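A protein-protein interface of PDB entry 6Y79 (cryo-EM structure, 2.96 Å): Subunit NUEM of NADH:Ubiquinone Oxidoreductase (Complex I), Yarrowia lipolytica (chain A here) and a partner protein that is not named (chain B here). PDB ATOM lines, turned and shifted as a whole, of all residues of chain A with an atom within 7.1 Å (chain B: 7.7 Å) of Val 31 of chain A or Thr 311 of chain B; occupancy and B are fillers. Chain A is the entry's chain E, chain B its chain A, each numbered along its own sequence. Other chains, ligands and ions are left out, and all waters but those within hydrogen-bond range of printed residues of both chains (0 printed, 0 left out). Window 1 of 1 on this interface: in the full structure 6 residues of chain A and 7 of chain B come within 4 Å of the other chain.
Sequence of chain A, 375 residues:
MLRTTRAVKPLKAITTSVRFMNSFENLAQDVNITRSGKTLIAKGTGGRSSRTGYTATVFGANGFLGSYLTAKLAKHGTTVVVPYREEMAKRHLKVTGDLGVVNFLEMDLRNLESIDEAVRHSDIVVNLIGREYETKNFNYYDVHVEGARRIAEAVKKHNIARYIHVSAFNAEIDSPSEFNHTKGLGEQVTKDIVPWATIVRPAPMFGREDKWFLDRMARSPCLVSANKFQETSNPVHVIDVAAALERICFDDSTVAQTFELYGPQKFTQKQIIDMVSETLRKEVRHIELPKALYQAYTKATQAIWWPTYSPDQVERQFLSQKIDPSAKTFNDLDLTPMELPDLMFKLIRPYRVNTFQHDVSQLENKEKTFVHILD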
ATOM      1  N   LEU A  27     -28.712  -8.131  38.511  1.00  0.00           N
ATOM      2  CA  LEU A  27     -27.940  -9.197  37.898  1.00  0.00           C
ATOM      3  C   LEU A  27     -26.828  -9.664  38.821  1.00  0.00           C
ATOM      4  O   LEU A  27     -26.189  -8.861  39.504  1.00  0.00           O
ATOM      5  CB  LEU A  27     -27.335  -8.718  36.582  1.00  0.00           C
ATOM      6  CG  LEU A  27     -28.261  -8.513  35.394  1.00  0.00           C
ATOM      7  CD1 LEU A  27     -27.439  -8.105  34.196  1.00  0.00           C
ATOM      8  CD2 LEU A  27     -29.028  -9.783  35.111  1.00  0.00           C
ATOM      9  N   GLN A  29     -24.268 -11.097  37.385  1.00  0.00           N
ATOM     10  CA  GLN A  29     -23.116 -11.012  36.494  1.00  0.00           C
ATOM     11  C   GLN A  29     -23.461 -10.136  35.301  1.00  0.00           C
ATOM     12  O   GLN A  29     -24.408  -9.349  35.324  1.00  0.00           O
ATOM     13  CB  GLN A  29     -22.695 -12.372  35.942  1.00  0.00           C
ATOM     14  CG  GLN A  29     -22.477 -13.474  36.899  1.00  0.00           C
ATOM     15  CD  GLN A  29     -22.247 -14.724  36.155  1.00  0.00           C
ATOM     16  OE1 GLN A  29     -22.119 -14.693  34.935  1.00  0.00           O
ATOM     17  NE2 GLN A  29     -22.209 -15.841  36.858  1.00  0.00           N
ATOM     18  N   ASP A  30     -22.653 -10.273  34.251  1.00  0.00           N
ATOM     19  CA  ASP A  30     -22.956  -9.745  32.927  1.00  0.00           C
ATOM     20  C   ASP A  30     -23.588 -10.820  32.040  1.00  0.00           C
ATOM     21  O   ASP A  30     -24.757 -10.710  31.662  1.00  0.00           O
ATOM     22  CB  ASP A  30     -21.659  -9.198  32.311  1.00  0.00           C
ATOM     23  CG  ASP A  30     -21.866  -8.452  30.995  1.00  0.00           C
ATOM     24  OD1 ASP A  30     -22.989  -8.407  30.451  1.00  0.00           O
ATOM     25  OD2 ASP A  30     -20.881  -7.866  30.504  1.00  0.00           O
ATOM     26  N   VAL A  31     -22.842 -11.869  31.722  1.00  0.00           N
ATOM     27  CA  VAL A  31     -23.286 -12.843  30.733  1.00  0.00           C
ATOM     28  C   VAL A  31     -24.168 -13.866  31.424  1.00  0.00           C
ATOM     29  O   VAL A  31     -23.708 -14.609  32.296  1.00  0.00           O
ATOM     30  CB  VAL A  31     -22.101 -13.521  30.036  1.00  0.00           C
ATOM     31  CG1 VAL A  31     -22.608 -14.577  29.072  1.00  0.00           C
ATOM     32  CG2 VAL A  31     -21.271 -12.496  29.297  1.00  0.00           C
ATOM     33  N   ASN A  32     -25.436 -13.903  31.039  1.00  0.00           N
ATOM     34  CA  ASN A  32     -26.404 -14.806  31.629  1.00  0.00           C
ATOM     35  C   ASN A  32     -27.005 -15.668  30.534  1.00  0.00           C
ATOM     36  O   ASN A  32     -27.475 -15.153  29.516  1.00  0.00           O
ATOM     37  CB  ASN A  32     -27.494 -14.030  32.361  1.00  0.00           C
ATOM     38  CG  ASN A  32     -26.972 -13.322  33.583  1.00  0.00           C
ATOM     39  OD1 ASN A  32     -27.033 -12.098  33.680  1.00  0.00           O
ATOM     40  ND2 ASN A  32     -26.444 -14.089  34.528  1.00  0.00           N
ATOM     41  N   ILE A  33     -26.976 -16.969  30.733  1.00  0.00           N
ATOM     42  CA  ILE A  33     -27.673 -17.892  29.852  1.00  0.00           C
ATOM     43  C   ILE A  33     -28.979 -18.276  30.534  1.00  0.00           C
ATOM     44  O   ILE A  33     -29.058 -18.342  31.768  1.00  0.00           O
ATOM     45  CB  ILE A  33     -26.792 -19.114  29.508  1.00  0.00           C
ATOM     46  CG1 ILE A  33     -27.423 -19.961  28.401  1.00  0.00           C
ATOM     47  CG2 ILE A  33     -26.465 -19.955  30.733  1.00  0.00           C
ATOM     48  CD1 ILE A  33     -26.475 -20.961  27.787  1.00  0.00           C
ATOM     49  N   THR A  39     -28.515 -17.015  24.941  1.00  0.00           N
ATOM     50  CA  THR A  39     -27.353 -16.358  25.524  1.00  0.00           C
ATOM     51  C   THR A  39     -27.615 -14.860  25.592  1.00  0.00           C
ATOM     52  O   THR A  39     -28.043 -14.261  24.602  1.00  0.00           O
ATOM     53  CB  THR A  39     -26.104 -16.653  24.693  1.00  0.00           C
ATOM     54  OG1 THR A  39     -25.844 -18.063  24.711  1.00  0.00           O
ATOM     55  CG2 THR A  39     -24.890 -15.914  25.237  1.00  0.00           C
ATOM     56  N   LEU A  40     -27.364 -14.255  26.754  1.00  0.00           N
ATOM     57  CA  LEU A  40     -27.761 -12.881  27.030  1.00  0.00           C
ATOM     58  C   LEU A  40     -26.552 -12.129  27.560  1.00  0.00           C
ATOM     59  O   LEU A  40     -26.134 -12.346  28.700  1.00  0.00           O
ATOM     60  CB  LEU A  40     -28.899 -12.837  28.048  1.00  0.00           C
ATOM     61  CG  LEU A  40     -30.358 -13.034  27.645  1.00  0.00           C
ATOM     62  CD1 LEU A  40     -30.673 -14.444  27.228  1.00  0.00           C
ATOM     63  CD2 LEU A  40     -31.190 -12.698  28.830  1.00  0.00           C
ATOM     64  N   ILE A  41     -25.998 -11.243  26.747  1.00  0.00           N
ATOM     65  CA  ILE A  41     -24.887 -10.396  27.154  1.00  0.00           C
ATOM     66  C   ILE A  41     -25.463  -9.031  27.493  1.00  0.00           C
ATOM     67  O   ILE A  41     -26.003  -8.348  26.621  1.00  0.00           O
ATOM     68  CB  ILE A  41     -23.828 -10.292  26.053  1.00  0.00           C
ATOM     69  CG1 ILE A  41     -23.276 -11.675  25.712  1.00  0.00           C
ATOM     70  CG2 ILE A  41     -22.718  -9.367  26.482  1.00  0.00           C
ATOM     71  CD1 ILE A  41     -22.426 -11.681  24.475  1.00  0.00           C
ATOM     72  N   ALA A  42     -25.372  -8.629  28.755  1.00  0.00           N
ATOM     73  CA  ALA A  42     -25.864  -7.313  29.131  1.00  0.00           C
ATOM     74  C   ALA A  42     -24.882  -6.245  28.675  1.00  0.00           C
ATOM     75  O   ALA A  42     -23.675  -6.473  28.595  1.00  0.00           O
ATOM     76  CB  ALA A  42     -26.093  -7.230  30.637  1.00  0.00           C
ATOM     77  N   TYR A  54     -32.894  -9.573  28.973  1.00  0.00           N
ATOM     78  CA  TYR A  54     -34.082 -10.375  29.225  1.00  0.00           C
ATOM     79  C   TYR A  54     -35.305  -9.757  28.569  1.00  0.00           C
ATOM     80  O   TYR A  54     -35.426  -8.534  28.469  1.00  0.00           O
ATOM     81  CB  TYR A  54     -34.334 -10.497  30.723  1.00  0.00           C
ATOM     82  CG  TYR A  54     -33.316 -11.309  31.479  1.00  0.00           C
ATOM     83  CD1 TYR A  54     -33.446 -12.688  31.596  1.00  0.00           C
ATOM     84  CD2 TYR A  54     -32.241 -10.695  32.099  1.00  0.00           C
ATOM     85  CE1 TYR A  54     -32.517 -13.431  32.291  1.00  0.00           C
ATOM     86  CE2 TYR A  54     -31.313 -11.425  32.798  1.00  0.00           C
ATOM     87  CZ  TYR A  54     -31.455 -12.791  32.892  1.00  0.00           C
ATOM     88  OH  TYR A  54     -30.529 -13.526  33.592  1.00  0.00           O
ATOM     89  N   ARG B 308     -14.463 -13.534  16.298  1.00  0.00           N
ATOM     90  CA  ARG B 308     -14.029 -13.266  17.655  1.00  0.00           C
ATOM     91  C   ARG B 308     -14.764 -14.119  18.679  1.00  0.00           C
ATOM     92  O   ARG B 308     -15.920 -14.506  18.501  1.00  0.00           O
ATOM     93  CB  ARG B 308     -14.252 -11.808  18.007  1.00  0.00           C
ATOM     94  CG  ARG B 308     -13.441 -10.844  17.223  1.00  0.00           C
ATOM     95  CD  ARG B 308     -13.793  -9.501  17.745  1.00  0.00           C
ATOM     96  NE  ARG B 308     -13.399  -9.373  19.136  1.00  0.00           N
ATOM     97  CZ  ARG B 308     -12.222  -8.915  19.537  1.00  0.00           C
ATOM     98  NH1 ARG B 308     -11.317  -8.531  18.650  1.00  0.00           N
ATOM     99  NH2 ARG B 308     -11.957  -8.833  20.830  1.00  0.00           N
ATOM    100  N   LEU B 309     -14.081 -14.359  19.792  1.00  0.00           N
ATOM    101  CA  LEU B 309     -14.667 -14.974  20.972  1.00  0.00           C
ATOM    102  C   LEU B 309     -15.302 -13.886  21.826  1.00  0.00           C
ATOM    103  O   LEU B 309     -14.634 -12.913  22.189  1.00  0.00           O
ATOM    104  CB  LEU B 309     -13.599 -15.725  21.767  1.00  0.00           C
ATOM    105  CG  LEU B 309     -12.966 -16.898  21.023  1.00  0.00           C
ATOM    106  CD1 LEU B 309     -11.804 -17.476  21.802  1.00  0.00           C
ATOM    107  CD2 LEU B 309     -14.007 -17.956  20.767  1.00  0.00           C
ATOM    108  N   THR B 310     -16.592 -14.041  22.130  1.00  0.00           N
ATOM    109  CA  THR B 310     -17.329 -13.055  22.914  1.00  0.00           C
ATOM    110  C   THR B 310     -17.919 -13.622  24.197  1.00  0.00           C
ATOM    111  O   THR B 310     -18.604 -12.888  24.918  1.00  0.00           O
ATOM    112  CB  THR B 310     -18.464 -12.439  22.084  1.00  0.00           C
ATOM    113  OG1 THR B 310     -19.389 -13.464  21.703  1.00  0.00           O
ATOM    114  CG2 THR B 310     -17.927 -11.760  20.835  1.00  0.00           C
ATOM    115  N   THR B 311     -17.677 -14.891  24.502  1.00  0.00           N
ATOM    116  CA  THR B 311     -18.266 -15.569  25.647  1.00  0.00           C
ATOM    117  C   THR B 311     -17.401 -16.794  25.929  1.00  0.00           C
ATOM    118  O   THR B 311     -16.691 -17.245  25.030  1.00  0.00           O
ATOM    119  CB  THR B 311     -19.732 -15.951  25.350  1.00  0.00           C
ATOM    120  OG1 THR B 311     -20.367 -16.506  26.510  1.00  0.00           O
ATOM    121  CG2 THR B 311     -19.833 -16.910  24.175  1.00  0.00           C
ATOM    122  N   PRO B 312     -17.364 -17.284  27.165  1.00  0.00           N
ATOM    123  CA  PRO B 312     -16.615 -18.522  27.416  1.00  0.00           C
ATOM    124  C   PRO B 312     -17.388 -19.740  26.944  1.00  0.00           C
ATOM    125  O   PRO B 312     -18.620 -19.771  26.952  1.00  0.00           O
ATOM    126  CB  PRO B 312     -16.441 -18.529  28.939  1.00  0.00           C
ATOM    127  CG  PRO B 312     -17.558 -17.713  29.445  1.00  0.00           C
ATOM    128  CD  PRO B 312     -17.779 -16.643  28.423  1.00  0.00           C
ATOM    129  N   LEU B 313     -16.643 -20.756  26.518  1.00  0.00           N
ATOM    130  CA  LEU B 313     -17.273 -21.963  26.003  1.00  0.00           C
ATOM    131  C   LEU B 313     -16.697 -23.191  26.680  1.00  0.00           C
ATOM    132  O   LEU B 313     -15.493 -23.263  26.942  1.00  0.00           O
ATOM    133  CB  LEU B 313     -17.095 -22.110  24.502  1.00  0.00           C
ATOM    134  CG  LEU B 313     -17.918 -21.343  23.476  1.00  0.00           C
ATOM    135  CD1 LEU B 313     -17.538 -19.896  23.381  1.00  0.00           C
ATOM    136  CD2 LEU B 313     -17.645 -21.990  22.174  1.00  0.00           C
ATOM    137  N   ILE B 314     -17.568 -24.163  26.933  1.00  0.00           N
ATOM    138  CA  ILE B 314     -17.211 -25.414  27.581  1.00  0.00           C
ATOM    139  C   ILE B 314     -17.541 -26.555  26.631  1.00  0.00           C
ATOM    140  O   ILE B 314     -18.629 -26.591  26.041  1.00  0.00           O
ATOM    141  CB  ILE B 314     -17.934 -25.571  28.930  1.00  0.00           C
ATOM    142  CG1 ILE B 314     -17.487 -24.461  29.875  1.00  0.00           C
ATOM    143  CG2 ILE B 314     -17.651 -26.924  29.565  1.00  0.00           C
ATOM    144  CD1 ILE B 314     -18.262 -24.403  31.127  1.00  0.00           C
ATOM    145  N   VAL B 321     -20.561 -25.800  23.975  1.00  0.00           N
ATOM    146  CA  VAL B 321     -21.679 -24.935  24.323  1.00  0.00           C
ATOM    147  C   VAL B 321     -21.087 -23.658  24.899  1.00  0.00           C
ATOM    148  O   VAL B 321     -19.965 -23.658  25.414  1.00  0.00           O
ATOM    149  CB  VAL B 321     -22.676 -25.583  25.320  1.00  0.00           C
ATOM    150  CG1 VAL B 321     -23.343 -26.810  24.711  1.00  0.00           C
ATOM    151  CG2 VAL B 321     -21.994 -25.933  26.635  1.00  0.00           C
ATOM    152  N   ASN B 322     -21.814 -22.552  24.773  1.00  0.00           N
ATOM    153  CA  ASN B 322     -21.334 -21.356  25.448  1.00  0.00           C
ATOM    154  C   ASN B 322     -21.886 -21.327  26.867  1.00  0.00           C
ATOM    155  O   ASN B 322     -22.868 -21.999  27.187  1.00  0.00           O
ATOM    156  CB  ASN B 322     -21.663 -20.070  24.670  1.00  0.00           C
ATOM    157  CG  ASN B 322     -23.159 -19.818  24.457  1.00  0.00           C
ATOM    158  OD1 ASN B 322     -24.031 -20.536  24.945  1.00  0.00           O
ATOM    159  ND2 ASN B 322     -23.452 -18.763  23.705  1.00  0.00           N
ATOM    160  N   ALA B 323     -21.231 -20.562  27.730  1.00  0.00           N
ATOM    161  CA  ALA B 323     -21.514 -20.733  29.141  1.00  0.00           C
ATOM    162  C   ALA B 323     -21.312 -19.446  29.920  1.00  0.00           C
ATOM    163  O   ALA B 323     -20.859 -18.421  29.406  1.00  0.00           O
ATOM    164  CB  ALA B 323     -20.654 -21.843  29.747  1.00  0.00           C
ATOM    165  N   THR B 324     -21.682 -19.550  31.186  1.00  0.00           N
ATOM    166  CA  THR B 324     -21.536 -18.559  32.231  1.00  0.00           C
ATOM    167  C   THR B 324     -20.067 -18.478  32.665  1.00  0.00           C
ATOM    168  O   THR B 324     -19.295 -19.429  32.504  1.00  0.00           O
ATOM    169  CB  THR B 324     -22.496 -18.974  33.360  1.00  0.00           C
ATOM    170  OG1 THR B 324     -23.838 -18.966  32.859  1.00  0.00           O
ATOM    171  CG2 THR B 324     -22.442 -18.122  34.589  1.00  0.00           C
ATOM    172  N   TRP B 325     -19.665 -17.298  33.162  1.00  0.00           N
ATOM    173  CA  TRP B 325     -18.326 -17.122  33.722  1.00  0.00           C
ATOM    174  C   TRP B 325     -18.093 -18.023  34.925  1.00  0.00           C
ATOM    175  O   TRP B 325     -17.027 -18.639  35.046  1.00  0.00           O
ATOM    176  CB  TRP B 325     -18.117 -15.664  34.109  1.00  0.00           C
ATOM    177  CG  TRP B 325     -18.041 -14.852  32.921  1.00  0.00           C
ATOM    178  CD1 TRP B 325     -19.036 -14.106  32.371  1.00  0.00           C
ATOM    179  CD2 TRP B 325     -16.923 -14.749  32.048  1.00  0.00           C
ATOM    180  NE1 TRP B 325     -18.592 -13.515  31.218  1.00  0.00           N
ATOM    181  CE2 TRP B 325     -17.295 -13.898  31.001  1.00  0.00           C
ATOM    182  CE3 TRP B 325     -15.629 -15.282  32.059  1.00  0.00           C
ATOM    183  CZ2 TRP B 325     -16.433 -13.579  29.974  1.00  0.00           C
ATOM    184  CZ3 TRP B 325     -14.768 -14.950  31.035  1.00  0.00           C
ATOM    185  CH2 TRP B 325     -15.173 -14.102  30.010  1.00  0.00           C
ATOM    186  N   ASP B 326     -19.068 -18.083  35.835  1.00  0.00           N
ATOM    187  CA  ASP B 326     -18.988 -18.986  36.980  1.00  0.00           C
ATOM    188  C   ASP B 326     -18.901 -20.434  36.516  1.00  0.00           C
ATOM    189  O   ASP B 326     -18.127 -21.218  37.071  1.00  0.00           O
ATOM    190  CB  ASP B 326     -20.206 -18.773  37.892  1.00  0.00           C
ATOM    191  CG  ASP B 326     -20.056 -19.418  39.277  1.00  0.00           C
ATOM    192  OD1 ASP B 326     -19.014 -20.055  39.558  1.00  0.00           O
ATOM    193  OD2 ASP B 326     -20.986 -19.283  40.101  1.00  0.00           O
ATOM    194  N   ALA B 328     -17.584 -21.567  33.539  1.00  0.00           N
ATOM    195  CA  ALA B 328     -16.282 -21.868  32.940  1.00  0.00           C
ATOM    196  C   ALA B 328     -15.169 -21.882  33.982  1.00  0.00           C
ATOM    197  O   ALA B 328     -14.355 -22.817  34.029  1.00  0.00           O
ATOM    198  CB  ALA B 328     -15.966 -20.859  31.835  1.00  0.00           C
ATOM    199  N   GLY B 573      -7.920 -16.634  24.711  1.00  0.00           N
ATOM    200  CA  GLY B 573      -7.542 -15.922  23.503  1.00  0.00           C
ATOM    201  C   GLY B 573      -8.703 -15.093  23.017  1.00  0.00           C
ATOM    202  O   GLY B 573      -9.834 -15.240  23.480  1.00  0.00           O
ATOM    203  N   VAL B 586     -12.741 -22.474  26.446  1.00  0.00           N
ATOM    204  CA  VAL B 586     -12.116 -21.277  25.892  1.00  0.00           C
ATOM    205  C   VAL B 586     -12.642 -20.053  26.628  1.00  0.00           C
ATOM    206  O   VAL B 586     -13.808 -19.983  27.040  1.00  0.00           O
ATOM    207  CB  VAL B 586     -12.286 -21.108  24.358  1.00  0.00           C
ATOM    208  CG1 VAL B 586     -11.650 -22.254  23.612  1.00  0.00           C
ATOM    209  CG2 VAL B 586     -13.723 -20.954  23.953  1.00  0.00           C
ATOM    210  N   LEU B 587     -11.740 -19.088  26.800  1.00  0.00           N
ATOM    211  CA  LEU B 587     -11.990 -17.861  27.545  1.00  0.00           C
ATOM    212  C   LEU B 587     -11.662 -16.679  26.644  1.00  0.00           C
ATOM    213  O   LEU B 587     -10.500 -16.547  26.193  1.00  0.00           O
ATOM    214  CB  LEU B 587     -11.156 -17.817  28.828  1.00  0.00           C
ATOM    215  CG  LEU B 587     -11.488 -18.847  29.908  1.00  0.00           C
ATOM    216  CD1 LEU B 587     -10.491 -18.771  31.052  1.00  0.00           C
ATOM    217  CD2 LEU B 587     -12.904 -18.643  30.416  1.00  0.00           C
ATOM    218  N   PRO B 588     -12.619 -15.798  26.367  1.00  0.00           N
ATOM    219  CA  PRO B 588     -12.348 -14.663  25.480  1.00  0.00           C
ATOM    220  C   PRO B 588     -11.501 -13.603  26.163  1.00  0.00           C
ATOM    221  O   PRO B 588     -11.727 -13.252  27.321  1.00  0.00           O
ATOM    222  CB  PRO B 588     -13.744 -14.132  25.152  1.00  0.00           C
ATOM    223  CG  PRO B 588     -14.571 -14.530  26.311  1.00  0.00           C
ATOM    224  CD  PRO B 588     -14.030 -15.843  26.786  1.00  0.00           C
ATOM    225  N   GLY B 589     -10.516 -13.086  25.428  1.00  0.00           N
ATOM    226  CA  GLY B 589      -9.662 -12.038  25.934  1.00  0.00           C
ATOM    227  C   GLY B 589      -9.744 -10.798  25.060  1.00  0.00           C
ATOM    228  O   GLY B 589     -10.335 -10.810  23.978  1.00  0.00           O
ATOM    229  N   PRO B 616     -15.502  -6.557  22.850  1.00  0.00           N
ATOM    230  CA  PRO B 616     -16.916  -6.713  22.518  1.00  0.00           C
ATOM    231  C   PRO B 616     -17.534  -7.953  23.135  1.00  0.00           C
ATOM    232  O   PRO B 616     -16.857  -8.936  23.442  1.00  0.00           O
ATOM    233  CB  PRO B 616     -16.911  -6.832  20.996  1.00  0.00           C
ATOM    234  CG  PRO B 616     -15.587  -7.422  20.696  1.00  0.00           C
ATOM    235  CD  PRO B 616     -14.631  -6.866  21.705  1.00  0.00           C
ATOM    236  N   GLY B 617     -18.858  -7.898  23.258  1.00  0.00           N
ATOM    237  CA  GLY B 617     -19.627  -8.959  23.867  1.00  0.00           C
ATOM    238  C   GLY B 617     -19.255  -9.119  25.320  1.00  0.00           C
ATOM    239  O   GLY B 617     -19.566  -8.264  26.153  1.00  0.00           O
ATOM    240  N   GLY B 618     -18.545 -10.197  25.625  1.00  0.00           N
ATOM    241  CA  GLY B 618     -18.159 -10.434  26.993  1.00  0.00           C
ATOM    242  C   GLY B 618     -16.678 -10.607  27.244  1.00  0.00           C
ATOM    243  O   GLY B 618     -16.328 -11.039  28.331  1.00  0.00           O
ATOM    244  N   ALA B 619     -15.800 -10.278  26.301  1.00  0.00           N
ATOM    245  CA  ALA B 619     -14.372 -10.469  26.531  1.00  0.00           C
ATOM    246  C   ALA B 619     -13.858  -9.510  27.604  1.00  0.00           C
ATOM    247  O   ALA B 619     -14.417  -8.435  27.824  1.00  0.00           O
ATOM    248  CB  ALA B 619     -13.591 -10.272  25.233  1.00  0.00           C
ATOM    249  N   ARG B 620     -12.810  -9.936  28.308  1.00  0.00           N
ATOM    250  CA  ARG B 620     -12.180  -9.134  29.349  1.00  0.00           C
ATOM    251  C   ARG B 620     -10.685  -9.011  29.103  1.00  0.00           C
ATOM    252  O   ARG B 620     -10.131  -9.550  28.141  1.00  0.00           O
ATOM    253  CB  ARG B 620     -12.389  -9.725  30.750  1.00  0.00           C
ATOM    254  CG  ARG B 620     -13.744  -9.494  31.377  1.00  0.00           C
ATOM    255  CD  ARG B 620     -14.651 -10.628  31.025  1.00  0.00           C
ATOM    256  NE  ARG B 620     -15.926 -10.609  31.725  1.00  0.00           N
ATOM    257  CZ  ARG B 620     -17.002  -9.986  31.267  1.00  0.00           C
ATOM    258  NH1 ARG B 620     -16.936  -9.303  30.134  1.00  0.00           N
ATOM    259  NH2 ARG B 620     -18.136 -10.029  31.946  1.00  0.00           N
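Hydrophobic or aromatic side chains of chain B that line the printed part of chain A: Trp 325. Hydrophobic or aromatic side chains of chain A within 4 Å of the printed part of chain B: Val 31, Ile 33 and Ile 41. Among the printed residues, Asp or Glu carboxylates within 4 Å of a Lys or Arg side-chain nitrogen of the other chain: Asp 30 of chain A with Arg 620 of chain B.
Among the printed residues, merely in contact across the chains: Gln 29 of chain A with Thr 324 of chain B, Ile 41 of chain A with Gly 617 of chain B, Val 31 of chain A with Trp 325 of chain B, Ile 33 of chain A with Thr 324 of chain B, Gln 29 of chain A with Asp 326 of chain B, Ile 33 of chain A with Asn 322 of chain B, Val 31 of chain A with Thr 311 of chain B and Gln 29 of chain A with Trp 325 of chain B.
The side-chain carboxylate (OD1) of Asp 30 of chain A sits at hydrogen-bond distance from the backbone NH (N) of Ala 42 of chain A, 2.9 Å away. O of Asp 30 of chain A sits close to OD1 of Asn 32 of chain A (3.3 Å). OE1 of Gln 29 of chain A sits close to O of Val 31 of chain A, 3.1 Å away. O of Gly 618 of chain B lies within hydrogen-bond range of NH1 of Arg 620 of chain B, at 2.6 Å.
Of the printed residues of chain B, Gln 29 of chain A touches Thr 324 (3.2 Å), Trp 325 (3.99 Å) and Asp 326 (3.7 Å). Val 31 of chain A touches two residues of chain B. Printed residues of chain A within 4 Å of Thr 311 of chain B: Val 31 (3.9 Å). Of the printed residues of chain A, Trp 325 of chain B touches Gln 29 and Val 31. Of the printed residues of chain A, Asp 326 of chain B touches Gln 29. Pro 588 of chain B touches none of the printed residues of chain A. Of the printed residues of chain A, Arg 620 of chain B touches Asp 30. The nearest printed residue of chain B that does not touch Thr 39 of chain A is Thr 311 of chain B (4.7 Å).
NH2 of Arg 620 of chain B lies within salt-bridge range of OD2 of Asp 30 of chain A, 3.8 Å away. OG1 of Thr 39 of chain A sits at hydrogen-bond distance from ND2 of Asn 322 of chain B.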
